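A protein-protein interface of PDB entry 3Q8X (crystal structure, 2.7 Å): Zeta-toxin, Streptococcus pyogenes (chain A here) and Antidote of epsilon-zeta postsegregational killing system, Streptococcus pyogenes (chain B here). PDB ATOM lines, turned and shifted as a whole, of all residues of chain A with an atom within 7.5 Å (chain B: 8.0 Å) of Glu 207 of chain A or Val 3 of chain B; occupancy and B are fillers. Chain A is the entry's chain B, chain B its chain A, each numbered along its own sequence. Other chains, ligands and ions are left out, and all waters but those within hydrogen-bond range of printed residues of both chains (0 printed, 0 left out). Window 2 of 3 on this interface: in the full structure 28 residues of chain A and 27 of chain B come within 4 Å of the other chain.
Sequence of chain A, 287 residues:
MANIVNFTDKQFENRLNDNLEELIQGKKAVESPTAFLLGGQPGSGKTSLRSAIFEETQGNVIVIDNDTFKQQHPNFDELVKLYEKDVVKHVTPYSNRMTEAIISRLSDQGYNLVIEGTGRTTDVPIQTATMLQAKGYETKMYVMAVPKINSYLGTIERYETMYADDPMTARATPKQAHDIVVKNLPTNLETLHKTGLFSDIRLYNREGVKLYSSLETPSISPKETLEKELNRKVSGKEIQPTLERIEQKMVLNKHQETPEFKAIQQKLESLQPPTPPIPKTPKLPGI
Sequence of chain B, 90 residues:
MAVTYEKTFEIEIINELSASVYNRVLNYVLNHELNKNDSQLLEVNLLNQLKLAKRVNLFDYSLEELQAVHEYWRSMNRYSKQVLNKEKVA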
ATOM      1  N   GLY A  45       1.430  15.270  19.571  1.00  0.00           N
ATOM      2  CA  GLY A  45       2.066  15.516  20.863  1.00  0.00           C
ATOM      3  C   GLY A  45       3.233  14.597  21.150  1.00  0.00           C
ATOM      4  O   GLY A  45       3.454  14.201  22.299  1.00  0.00           O
ATOM      5  N   THR A  47       6.198  14.963  21.703  1.00  0.00           N
ATOM      6  CA  THR A  47       7.039  15.323  22.844  1.00  0.00           C
ATOM      7  C   THR A  47       6.730  14.428  24.058  1.00  0.00           C
ATOM      8  O   THR A  47       7.613  14.147  24.857  1.00  0.00           O
ATOM      9  CB  THR A  47       6.952  16.820  23.173  1.00  0.00           C
ATOM     10  OG1 THR A  47       7.379  17.562  22.027  1.00  0.00           O
ATOM     11  CG2 THR A  47       7.865  17.183  24.329  1.00  0.00           C
ATOM     12  N   SER A  48       5.496  13.937  24.164  1.00  0.00           N
ATOM     13  CA  SER A  48       5.160  12.925  25.167  1.00  0.00           C
ATOM     14  C   SER A  48       6.044  11.684  25.088  1.00  0.00           C
ATOM     15  O   SER A  48       6.381  11.089  26.112  1.00  0.00           O
ATOM     16  CB  SER A  48       3.689  12.521  25.073  1.00  0.00           C
ATOM     17  OG  SER A  48       2.897  13.336  25.928  1.00  0.00           O
ATOM     18  N   LEU A  49       6.426  11.301  23.873  1.00  0.00           N
ATOM     19  CA  LEU A  49       7.278  10.138  23.677  1.00  0.00           C
ATOM     20  C   LEU A  49       8.686  10.390  24.207  1.00  0.00           C
ATOM     21  O   LEU A  49       9.256   9.539  24.898  1.00  0.00           O
ATOM     22  CB  LEU A  49       7.307   9.741  22.208  1.00  0.00           C
ATOM     23  CG  LEU A  49       5.942   9.459  21.591  1.00  0.00           C
ATOM     24  CD1 LEU A  49       6.109   9.266  20.117  1.00  0.00           C
ATOM     25  CD2 LEU A  49       5.294   8.246  22.201  1.00  0.00           C
ATOM     26  N   SER A  51       9.451  12.186  26.613  1.00  0.00           N
ATOM     27  CA  SER A  51       9.366  12.083  28.053  1.00  0.00           C
ATOM     28  C   SER A  51       9.590  10.645  28.518  1.00  0.00           C
ATOM     29  O   SER A  51      10.486  10.390  29.321  1.00  0.00           O
ATOM     30  CB  SER A  51       8.035  12.623  28.562  1.00  0.00           C
ATOM     31  OG  SER A  51       7.961  12.489  29.970  1.00  0.00           O
ATOM     32  N   ALA A  52       8.793   9.716  27.993  1.00  0.00           N
ATOM     33  CA  ALA A  52       8.870   8.303  28.378  1.00  0.00           C
ATOM     34  C   ALA A  52      10.255   7.705  28.130  1.00  0.00           C
ATOM     35  O   ALA A  52      10.778   6.963  28.972  1.00  0.00           O
ATOM     36  CB  ALA A  52       7.801   7.495  27.646  1.00  0.00           C
ATOM     37  N   GLU A  55      12.817   8.989  30.620  1.00  0.00           N
ATOM     38  CA  GLU A  55      12.659   8.193  31.831  1.00  0.00           C
ATOM     39  C   GLU A  55      13.308   6.814  31.630  1.00  0.00           C
ATOM     40  O   GLU A  55      14.126   6.383  32.438  1.00  0.00           O
ATOM     41  CB  GLU A  55      11.173   8.044  32.129  1.00  0.00           C
ATOM     42  CG  GLU A  55      10.751   8.331  33.552  1.00  0.00           C
ATOM     43  CD  GLU A  55       9.218   8.223  33.751  1.00  0.00           C
ATOM     44  OE1 GLU A  55       8.460   8.416  32.759  1.00  0.00           O
ATOM     45  OE2 GLU A  55       8.775   7.942  34.904  1.00  0.00           O
ATOM     46  N   MET A 144       2.633   7.826  18.647  1.00  0.00           N
ATOM     47  CA  MET A 144       1.453   8.433  19.295  1.00  0.00           C
ATOM     48  C   MET A 144       0.170   7.930  18.647  1.00  0.00           C
ATOM     49  O   MET A 144       0.033   7.962  17.415  1.00  0.00           O
ATOM     50  CB  MET A 144       1.465   9.960  19.192  1.00  0.00           C
ATOM     51  CG  MET A 144       2.464  10.690  20.084  1.00  0.00           C
ATOM     52  SD  MET A 144       2.276  10.308  21.821  1.00  0.00           S
ATOM     53  CE  MET A 144       0.803  11.231  22.268  1.00  0.00           C
ATOM     54  N   ALA A 145      -0.767   7.473  19.475  1.00  0.00           N
ATOM     55  CA  ALA A 145      -2.104   7.163  19.013  1.00  0.00           C
ATOM     56  C   ALA A 145      -3.042   8.249  19.524  1.00  0.00           C
ATOM     57  O   ALA A 145      -3.399   8.266  20.702  1.00  0.00           O
ATOM     58  CB  ALA A 145      -2.532   5.808  19.512  1.00  0.00           C
ATOM     59  N   VAL A 146      -3.421   9.169  18.645  1.00  0.00           N
ATOM     60  CA  VAL A 146      -4.260  10.308  19.036  1.00  0.00           C
ATOM     61  C   VAL A 146      -5.354  10.536  18.004  1.00  0.00           C
ATOM     62  O   VAL A 146      -5.074  10.549  16.806  1.00  0.00           O
ATOM     63  CB  VAL A 146      -3.435  11.619  19.152  1.00  0.00           C
ATOM     64  CG1 VAL A 146      -4.344  12.808  19.381  1.00  0.00           C
ATOM     65  CG2 VAL A 146      -2.380  11.528  20.246  1.00  0.00           C
ATOM     66  N   ASN A 150      -8.259  15.688  17.757  1.00  0.00           N
ATOM     67  CA  ASN A 150      -7.354  16.194  18.798  1.00  0.00           C
ATOM     68  C   ASN A 150      -6.003  16.703  18.260  1.00  0.00           C
ATOM     69  O   ASN A 150      -5.489  17.744  18.692  1.00  0.00           O
ATOM     70  CB  ASN A 150      -7.134  15.129  19.879  1.00  0.00           C
ATOM     71  CG  ASN A 150      -8.255  15.094  20.907  1.00  0.00           C
ATOM     72  OD1 ASN A 150      -8.996  16.061  21.074  1.00  0.00           O
ATOM     73  ND2 ASN A 150      -8.373  13.981  21.608  1.00  0.00           N
ATOM     74  N   TYR A 204       1.441   5.070  22.398  1.00  0.00           N
ATOM     75  CA  TYR A 204       1.091   5.869  23.579  1.00  0.00           C
ATOM     76  C   TYR A 204      -0.037   6.829  23.269  1.00  0.00           C
ATOM     77  O   TYR A 204      -0.207   7.243  22.123  1.00  0.00           O
ATOM     78  CB  TYR A 204       2.284   6.667  24.089  1.00  0.00           C
ATOM     79  CG  TYR A 204       3.377   5.851  24.742  1.00  0.00           C
ATOM     80  CD1 TYR A 204       3.424   5.690  26.122  1.00  0.00           C
ATOM     81  CD2 TYR A 204       4.381   5.258  23.974  1.00  0.00           C
ATOM     82  CE1 TYR A 204       4.431   4.954  26.718  1.00  0.00           C
ATOM     83  CE2 TYR A 204       5.387   4.524  24.561  1.00  0.00           C
ATOM     84  CZ  TYR A 204       5.412   4.378  25.931  1.00  0.00           C
ATOM     85  OH  TYR A 204       6.426   3.647  26.507  1.00  0.00           O
ATOM     86  N   ASN A 205      -0.810   7.176  24.295  1.00  0.00           N
ATOM     87  CA  ASN A 205      -1.861   8.180  24.165  1.00  0.00           C
ATOM     88  C   ASN A 205      -1.444   9.508  24.774  1.00  0.00           C
ATOM     89  O   ASN A 205      -0.368   9.627  25.368  1.00  0.00           O
ATOM     90  CB  ASN A 205      -3.202   7.694  24.735  1.00  0.00           C
ATOM     91  CG  ASN A 205      -3.294   7.809  26.254  1.00  0.00           C
ATOM     92  OD1 ASN A 205      -2.312   8.071  26.957  1.00  0.00           O
ATOM     93  ND2 ASN A 205      -4.495   7.604  26.764  1.00  0.00           N
ATOM     94  N   ARG A 206      -2.299  10.509  24.625  1.00  0.00           N
ATOM     95  CA  ARG A 206      -1.940  11.857  25.040  1.00  0.00           C
ATOM     96  C   ARG A 206      -1.409  11.877  26.477  1.00  0.00           C
ATOM     97  O   ARG A 206      -0.433  12.572  26.772  1.00  0.00           O
ATOM     98  CB  ARG A 206      -3.140  12.787  24.870  1.00  0.00           C
ATOM     99  CG  ARG A 206      -2.759  14.243  24.744  1.00  0.00           C
ATOM    100  CD  ARG A 206      -3.775  15.019  23.936  1.00  0.00           C
ATOM    101  NE  ARG A 206      -3.281  15.238  22.581  1.00  0.00           N
ATOM    102  CZ  ARG A 206      -3.829  16.082  21.713  1.00  0.00           C
ATOM    103  NH1 ARG A 206      -4.898  16.777  22.060  1.00  0.00           N
ATOM    104  NH2 ARG A 206      -3.309  16.225  20.500  1.00  0.00           N
ATOM    105  N   GLU A 207      -2.034  11.072  27.340  1.00  0.00           N
ATOM    106  CA  GLU A 207      -1.754  11.051  28.777  1.00  0.00           C
ATOM    107  C   GLU A 207      -0.578  10.168  29.146  1.00  0.00           C
ATOM    108  O   GLU A 207      -0.360   9.897  30.325  1.00  0.00           O
ATOM    109  CB  GLU A 207      -2.989  10.600  29.553  1.00  0.00           C
ATOM    110  CG  GLU A 207      -4.081  11.650  29.638  1.00  0.00           C
ATOM    111  CD  GLU A 207      -4.684  11.971  28.286  1.00  0.00           C
ATOM    112  OE1 GLU A 207      -4.845  11.029  27.475  1.00  0.00           O
ATOM    113  OE2 GLU A 207      -4.986  13.160  28.025  1.00  0.00           O
ATOM    114  N   GLY A 208       0.175   9.722  28.141  1.00  0.00           N
ATOM    115  CA  GLY A 208       1.388   8.934  28.365  1.00  0.00           C
ATOM    116  C   GLY A 208       1.168   7.456  28.634  1.00  0.00           C
ATOM    117  O   GLY A 208       2.128   6.734  28.888  1.00  0.00           O
ATOM    118  N   VAL A 209      -0.089   7.004  28.577  1.00  0.00           N
ATOM    119  CA  VAL A 209      -0.442   5.598  28.796  1.00  0.00           C
ATOM    120  C   VAL A 209      -0.075   4.750  27.576  1.00  0.00           C
ATOM    121  O   VAL A 209      -0.529   5.028  26.459  1.00  0.00           O
ATOM    122  CB  VAL A 209      -1.964   5.420  29.097  1.00  0.00           C
ATOM    123  CG1 VAL A 209      -2.327   3.959  29.200  1.00  0.00           C
ATOM    124  CG2 VAL A 209      -2.372   6.146  30.364  1.00  0.00           C
ATOM    125  N   LYS A 210       0.737   3.716  27.812  1.00  0.00           N
ATOM    126  CA  LYS A 210       1.097   2.702  26.816  1.00  0.00           C
ATOM    127  C   LYS A 210      -0.121   1.846  26.446  1.00  0.00           C
ATOM    128  O   LYS A 210      -0.662   1.127  27.283  1.00  0.00           O
ATOM    129  CB  LYS A 210       2.206   1.821  27.390  1.00  0.00           C
ATOM    130  CG  LYS A 210       2.859   0.846  26.413  1.00  0.00           C
ATOM    131  CD  LYS A 210       3.391  -0.407  27.139  1.00  0.00           C
ATOM    132  CE  LYS A 210       4.673  -0.121  27.912  1.00  0.00           C
ATOM    133  NZ  LYS A 210       4.962  -1.151  28.949  1.00  0.00           N
ATOM    134  N   GLU A 229      -8.205   4.517  17.917  1.00  0.00           N
ATOM    135  CA  GLU A 229      -7.861   5.764  18.581  1.00  0.00           C
ATOM    136  C   GLU A 229      -7.925   6.974  17.648  1.00  0.00           C
ATOM    137  O   GLU A 229      -8.447   8.016  18.037  1.00  0.00           O
ATOM    138  CB  GLU A 229      -6.502   5.635  19.263  1.00  0.00           C
ATOM    139  CG  GLU A 229      -6.194   6.719  20.277  1.00  0.00           C
ATOM    140  CD  GLU A 229      -7.178   6.796  21.434  1.00  0.00           C
ATOM    141  OE1 GLU A 229      -7.800   5.767  21.808  1.00  0.00           O
ATOM    142  OE2 GLU A 229      -7.314   7.912  21.981  1.00  0.00           O
ATOM    143  N   ARG A 232     -11.658   7.402  17.095  1.00  0.00           N
ATOM    144  CA  ARG A 232     -12.511   7.567  18.268  1.00  0.00           C
ATOM    145  C   ARG A 232     -13.299   8.878  18.175  1.00  0.00           C
ATOM    146  O   ARG A 232     -12.742   9.933  17.850  1.00  0.00           O
ATOM    147  CB  ARG A 232     -11.678   7.513  19.553  1.00  0.00           C
ATOM    148  CG  ARG A 232     -12.474   7.665  20.850  1.00  0.00           C
ATOM    149  CD  ARG A 232     -11.650   7.254  22.089  1.00  0.00           C
ATOM    150  NE  ARG A 232     -10.455   8.074  22.341  1.00  0.00           N
ATOM    151  CZ  ARG A 232     -10.454   9.327  22.809  1.00  0.00           C
ATOM    152  NH1 ARG A 232     -11.590   9.971  23.068  1.00  0.00           N
ATOM    153  NH2 ARG A 232      -9.301   9.956  23.001  1.00  0.00           N
ATOM    154  N   GLU A 238     -14.798  16.957  25.903  1.00  0.00           N
ATOM    155  CA  GLU A 238     -13.362  16.689  25.881  1.00  0.00           C
ATOM    156  C   GLU A 238     -12.542  17.723  25.099  1.00  0.00           C
ATOM    157  O   GLU A 238     -11.386  17.982  25.437  1.00  0.00           O
ATOM    158  CB  GLU A 238     -13.059  15.276  25.374  1.00  0.00           C
ATOM    159  CG  GLU A 238     -11.647  14.795  25.723  1.00  0.00           C
ATOM    160  CD  GLU A 238     -11.175  13.625  24.873  1.00  0.00           C
ATOM    161  OE1 GLU A 238     -11.955  12.666  24.665  1.00  0.00           O
ATOM    162  OE2 GLU A 238     -10.004  13.661  24.421  1.00  0.00           O
ATOM    163  N   VAL B   3       3.403  13.535  33.193  1.00  0.00           N
ATOM    164  CA  VAL B   3       3.149  13.864  31.758  1.00  0.00           C
ATOM    165  C   VAL B   3       1.694  14.298  31.533  1.00  0.00           C
ATOM    166  O   VAL B   3       0.824  13.475  31.235  1.00  0.00           O
ATOM    167  CB  VAL B   3       3.496  12.664  30.832  1.00  0.00           C
ATOM    168  CG1 VAL B   3       3.276  13.014  29.355  1.00  0.00           C
ATOM    169  CG2 VAL B   3       4.934  12.203  31.064  1.00  0.00           C
ATOM    170  N   THR B   4       1.429  15.589  31.707  1.00  0.00           N
ATOM    171  CA  THR B   4       0.147  16.161  31.305  1.00  0.00           C
ATOM    172  C   THR B   4       0.359  16.730  29.924  1.00  0.00           C
ATOM    173  O   THR B   4       1.462  17.200  29.597  1.00  0.00           O
ATOM    174  CB  THR B   4      -0.311  17.300  32.220  1.00  0.00           C
ATOM    175  OG1 THR B   4       0.648  18.362  32.177  1.00  0.00           O
ATOM    176  CG2 THR B   4      -0.486  16.814  33.655  1.00  0.00           C
ATOM    177  N   TYR B   5      -0.687  16.690  29.108  1.00  0.00           N
ATOM    178  CA  TYR B   5      -0.610  17.266  27.770  1.00  0.00           C
ATOM    179  C   TYR B   5      -0.274  18.757  27.843  1.00  0.00           C
ATOM    180  O   TYR B   5       0.467  19.283  27.008  1.00  0.00           O
ATOM    181  CB  TYR B   5      -1.914  17.046  27.019  1.00  0.00           C
ATOM    182  CG  TYR B   5      -1.969  17.735  25.682  1.00  0.00           C
ATOM    183  CD1 TYR B   5      -1.114  17.360  24.643  1.00  0.00           C
ATOM    184  CD2 TYR B   5      -2.875  18.765  25.456  1.00  0.00           C
ATOM    185  CE1 TYR B   5      -1.170  17.991  23.418  1.00  0.00           C
ATOM    186  CE2 TYR B   5      -2.940  19.403  24.231  1.00  0.00           C
ATOM    187  CZ  TYR B   5      -2.086  19.014  23.217  1.00  0.00           C
ATOM    188  OH  TYR B   5      -2.156  19.658  22.003  1.00  0.00           O
ATOM    189  N   GLU B   6      -0.820  19.414  28.861  1.00  0.00           N
ATOM    190  CA  GLU B   6      -0.547  20.812  29.135  1.00  0.00           C
ATOM    191  C   GLU B   6       0.968  21.092  29.220  1.00  0.00           C
ATOM    192  O   GLU B   6       1.482  22.013  28.565  1.00  0.00           O
ATOM    193  CB  GLU B   6      -1.259  21.213  30.422  1.00  0.00           C
ATOM    194  CG  GLU B   6      -1.321  22.706  30.663  1.00  0.00           C
ATOM    195  CD  GLU B   6      -2.335  23.078  31.730  1.00  0.00           C
ATOM    196  OE1 GLU B   6      -3.028  22.175  32.252  1.00  0.00           O
ATOM    197  OE2 GLU B   6      -2.448  24.282  32.046  1.00  0.00           O
ATOM    198  N   LYS B   7       1.673  20.289  30.018  1.00  0.00           N
ATOM    199  CA  LYS B   7       3.125  20.404  30.124  1.00  0.00           C
ATOM    200  C   LYS B   7       3.792  19.967  28.832  1.00  0.00           C
ATOM    201  O   LYS B   7       4.648  20.681  28.325  1.00  0.00           O
ATOM    202  CB  LYS B   7       3.678  19.633  31.330  1.00  0.00           C
ATOM    203  CG  LYS B   7       3.261  20.233  32.674  1.00  0.00           C
ATOM    204  CD  LYS B   7       4.255  19.933  33.788  1.00  0.00           C
ATOM    205  CE  LYS B   7       4.040  18.544  34.401  1.00  0.00           C
ATOM    206  NZ  LYS B   7       4.964  18.331  35.559  1.00  0.00           N
ATOM    207  N   THR B   8       3.392  18.822  28.277  1.00  0.00           N
ATOM    208  CA  THR B   8       3.955  18.381  26.996  1.00  0.00           C
ATOM    209  C   THR B   8       3.884  19.501  25.954  1.00  0.00           C
ATOM    210  O   THR B   8       4.890  19.859  25.348  1.00  0.00           O
ATOM    211  CB  THR B   8       3.284  17.092  26.485  1.00  0.00           C
ATOM    212  OG1 THR B   8       3.721  15.982  27.282  1.00  0.00           O
ATOM    213  CG2 THR B   8       3.636  16.816  25.011  1.00  0.00           C
ATOM    214  N   PHE B   9       2.698  20.076  25.797  1.00  0.00           N
ATOM    215  CA  PHE B   9       2.482  21.183  24.879  1.00  0.00           C
ATOM    216  C   PHE B   9       3.433  22.350  25.116  1.00  0.00           C
ATOM    217  O   PHE B   9       4.063  22.843  24.175  1.00  0.00           O
ATOM    218  CB  PHE B   9       1.047  21.679  24.954  1.00  0.00           C
ATOM    219  CG  PHE B   9       0.699  22.628  23.865  1.00  0.00           C
ATOM    220  CD1 PHE B   9       0.802  23.996  24.065  1.00  0.00           C
ATOM    221  CD2 PHE B   9       0.294  22.146  22.614  1.00  0.00           C
ATOM    222  CE1 PHE B   9       0.500  24.872  23.041  1.00  0.00           C
ATOM    223  CE2 PHE B   9      -0.014  23.009  21.579  1.00  0.00           C
ATOM    224  CZ  PHE B   9       0.083  24.377  21.792  1.00  0.00           C
ATOM    225  N   ILE B  11       6.254  22.306  26.539  1.00  0.00           N
ATOM    226  CA  ILE B  11       7.590  21.870  26.174  1.00  0.00           C
ATOM    227  C   ILE B  11       7.782  21.883  24.647  1.00  0.00           C
ATOM    228  O   ILE B  11       8.833  22.300  24.170  1.00  0.00           O
ATOM    229  CB  ILE B  11       7.954  20.513  26.818  1.00  0.00           C
ATOM    230  CG1 ILE B  11       7.962  20.645  28.354  1.00  0.00           C
ATOM    231  CG2 ILE B  11       9.305  20.016  26.310  1.00  0.00           C
ATOM    232  CD1 ILE B  11       7.906  19.315  29.114  1.00  0.00           C
ATOM    233  N   PHE B  59      11.650  18.077  31.278  1.00  0.00           N
ATOM    234  CA  PHE B  59      10.664  17.087  31.725  1.00  0.00           C
ATOM    235  C   PHE B  59      10.579  17.031  33.241  1.00  0.00           C
ATOM    236  O   PHE B  59       9.638  16.480  33.797  1.00  0.00           O
ATOM    237  CB  PHE B  59      10.927  15.694  31.125  1.00  0.00           C
ATOM    238  CG  PHE B  59      10.910  15.676  29.629  1.00  0.00           C
ATOM    239  CD1 PHE B  59       9.735  15.946  28.932  1.00  0.00           C
ATOM    240  CD2 PHE B  59      12.073  15.410  28.910  1.00  0.00           C
ATOM    241  CE1 PHE B  59       9.721  15.952  27.536  1.00  0.00           C
ATOM    242  CE2 PHE B  59      12.075  15.416  27.517  1.00  0.00           C
ATOM    243  CZ  PHE B  59      10.901  15.689  26.828  1.00  0.00           C
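Among the printed residues, pairs that only touch across the chains: Gly 45 of chain A with Thr 8 of chain B (3.8 Å), Thr 47 of chain A with Thr 8 of chain B (3.8 Å), Thr 47 of chain A with Ile 11 of chain B (3.7 Å), Thr 47 of chain A with Phe 59 of chain B (3.9 Å), Ser 48 of chain A with Val 3 of chain B (3.5 Å), Ser 51 of chain A with Val 3 of chain B (3.2 Å), Ser 51 of chain A with Phe 59 of chain B (3.8 Å), Arg 206 of chain A with Tyr 5 of chain B (3.5 Å) and Glu 207 of chain A with Val 3 of chain B (3.9 Å).
Of chain A, only Ser 48, Ser 51 and Glu 207 come within 4 Å of Val 3 of chain B.
Printed residues of chain A within 4 Å of Thr 8 of chain B: Gly 45, Thr 47 and Ser 48.
Of the printed residues of chain A, Tyr 5 of chain B touches Arg 206 (3.5 Å).
Of the printed residues of chain B, Ser 51 of chain A touches Val 3 (3.2 Å) and Phe 59 (3.8 Å).
Of the printed residues of chain B, Ser 48 of chain A touches Val 3 and Thr 8.
Met 144 of chain A touches none of the printed residues of chain B.
The nearest residue of chain A that does not touch Val 3 of chain B is Arg 206 of chain A (4.5 Å).
The nearest printed residue of chain A that does not touch Phe 59 of chain B is Ser 48 of chain A (5.8 Å).
The backbone carbonyl oxygen (O) of Thr 4 of chain B is in hydrogen-bond range of the side-chain hydroxyl (OG1) of Thr 8 of chain B, at 3.5 Å.
The guanidinium group (NH2) of Arg 206 of chain A sits at hydrogen-bond distance from the backbone carbonyl oxygen (O) of Asn 150 of chain A, at 3.2 Å.
The side-chain amide oxygen (OD1) of Asn 205 of chain A is in hydrogen-bond range of the backbone NH (N) of Glu 207 of chain A (3.0 Å).
The side-chain hydroxyl of Thr 8 of chain B is in hydrogen-bond range of the side-chain hydroxyl of Ser 48 of chain A (3.1 Å).
Of the 21 printed residues of chain A, 6 touch a printed residue of chain B.
Along chain A the printed residues that touch a printed residue of chain B span positions 45 to 207.
Among the printed residues, 10 pairs touch across the chains.
Among the printed residues, no Asp or Glu carboxylate lies within 4 Å of a Lys or Arg side-chain nitrogen of the other chain.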
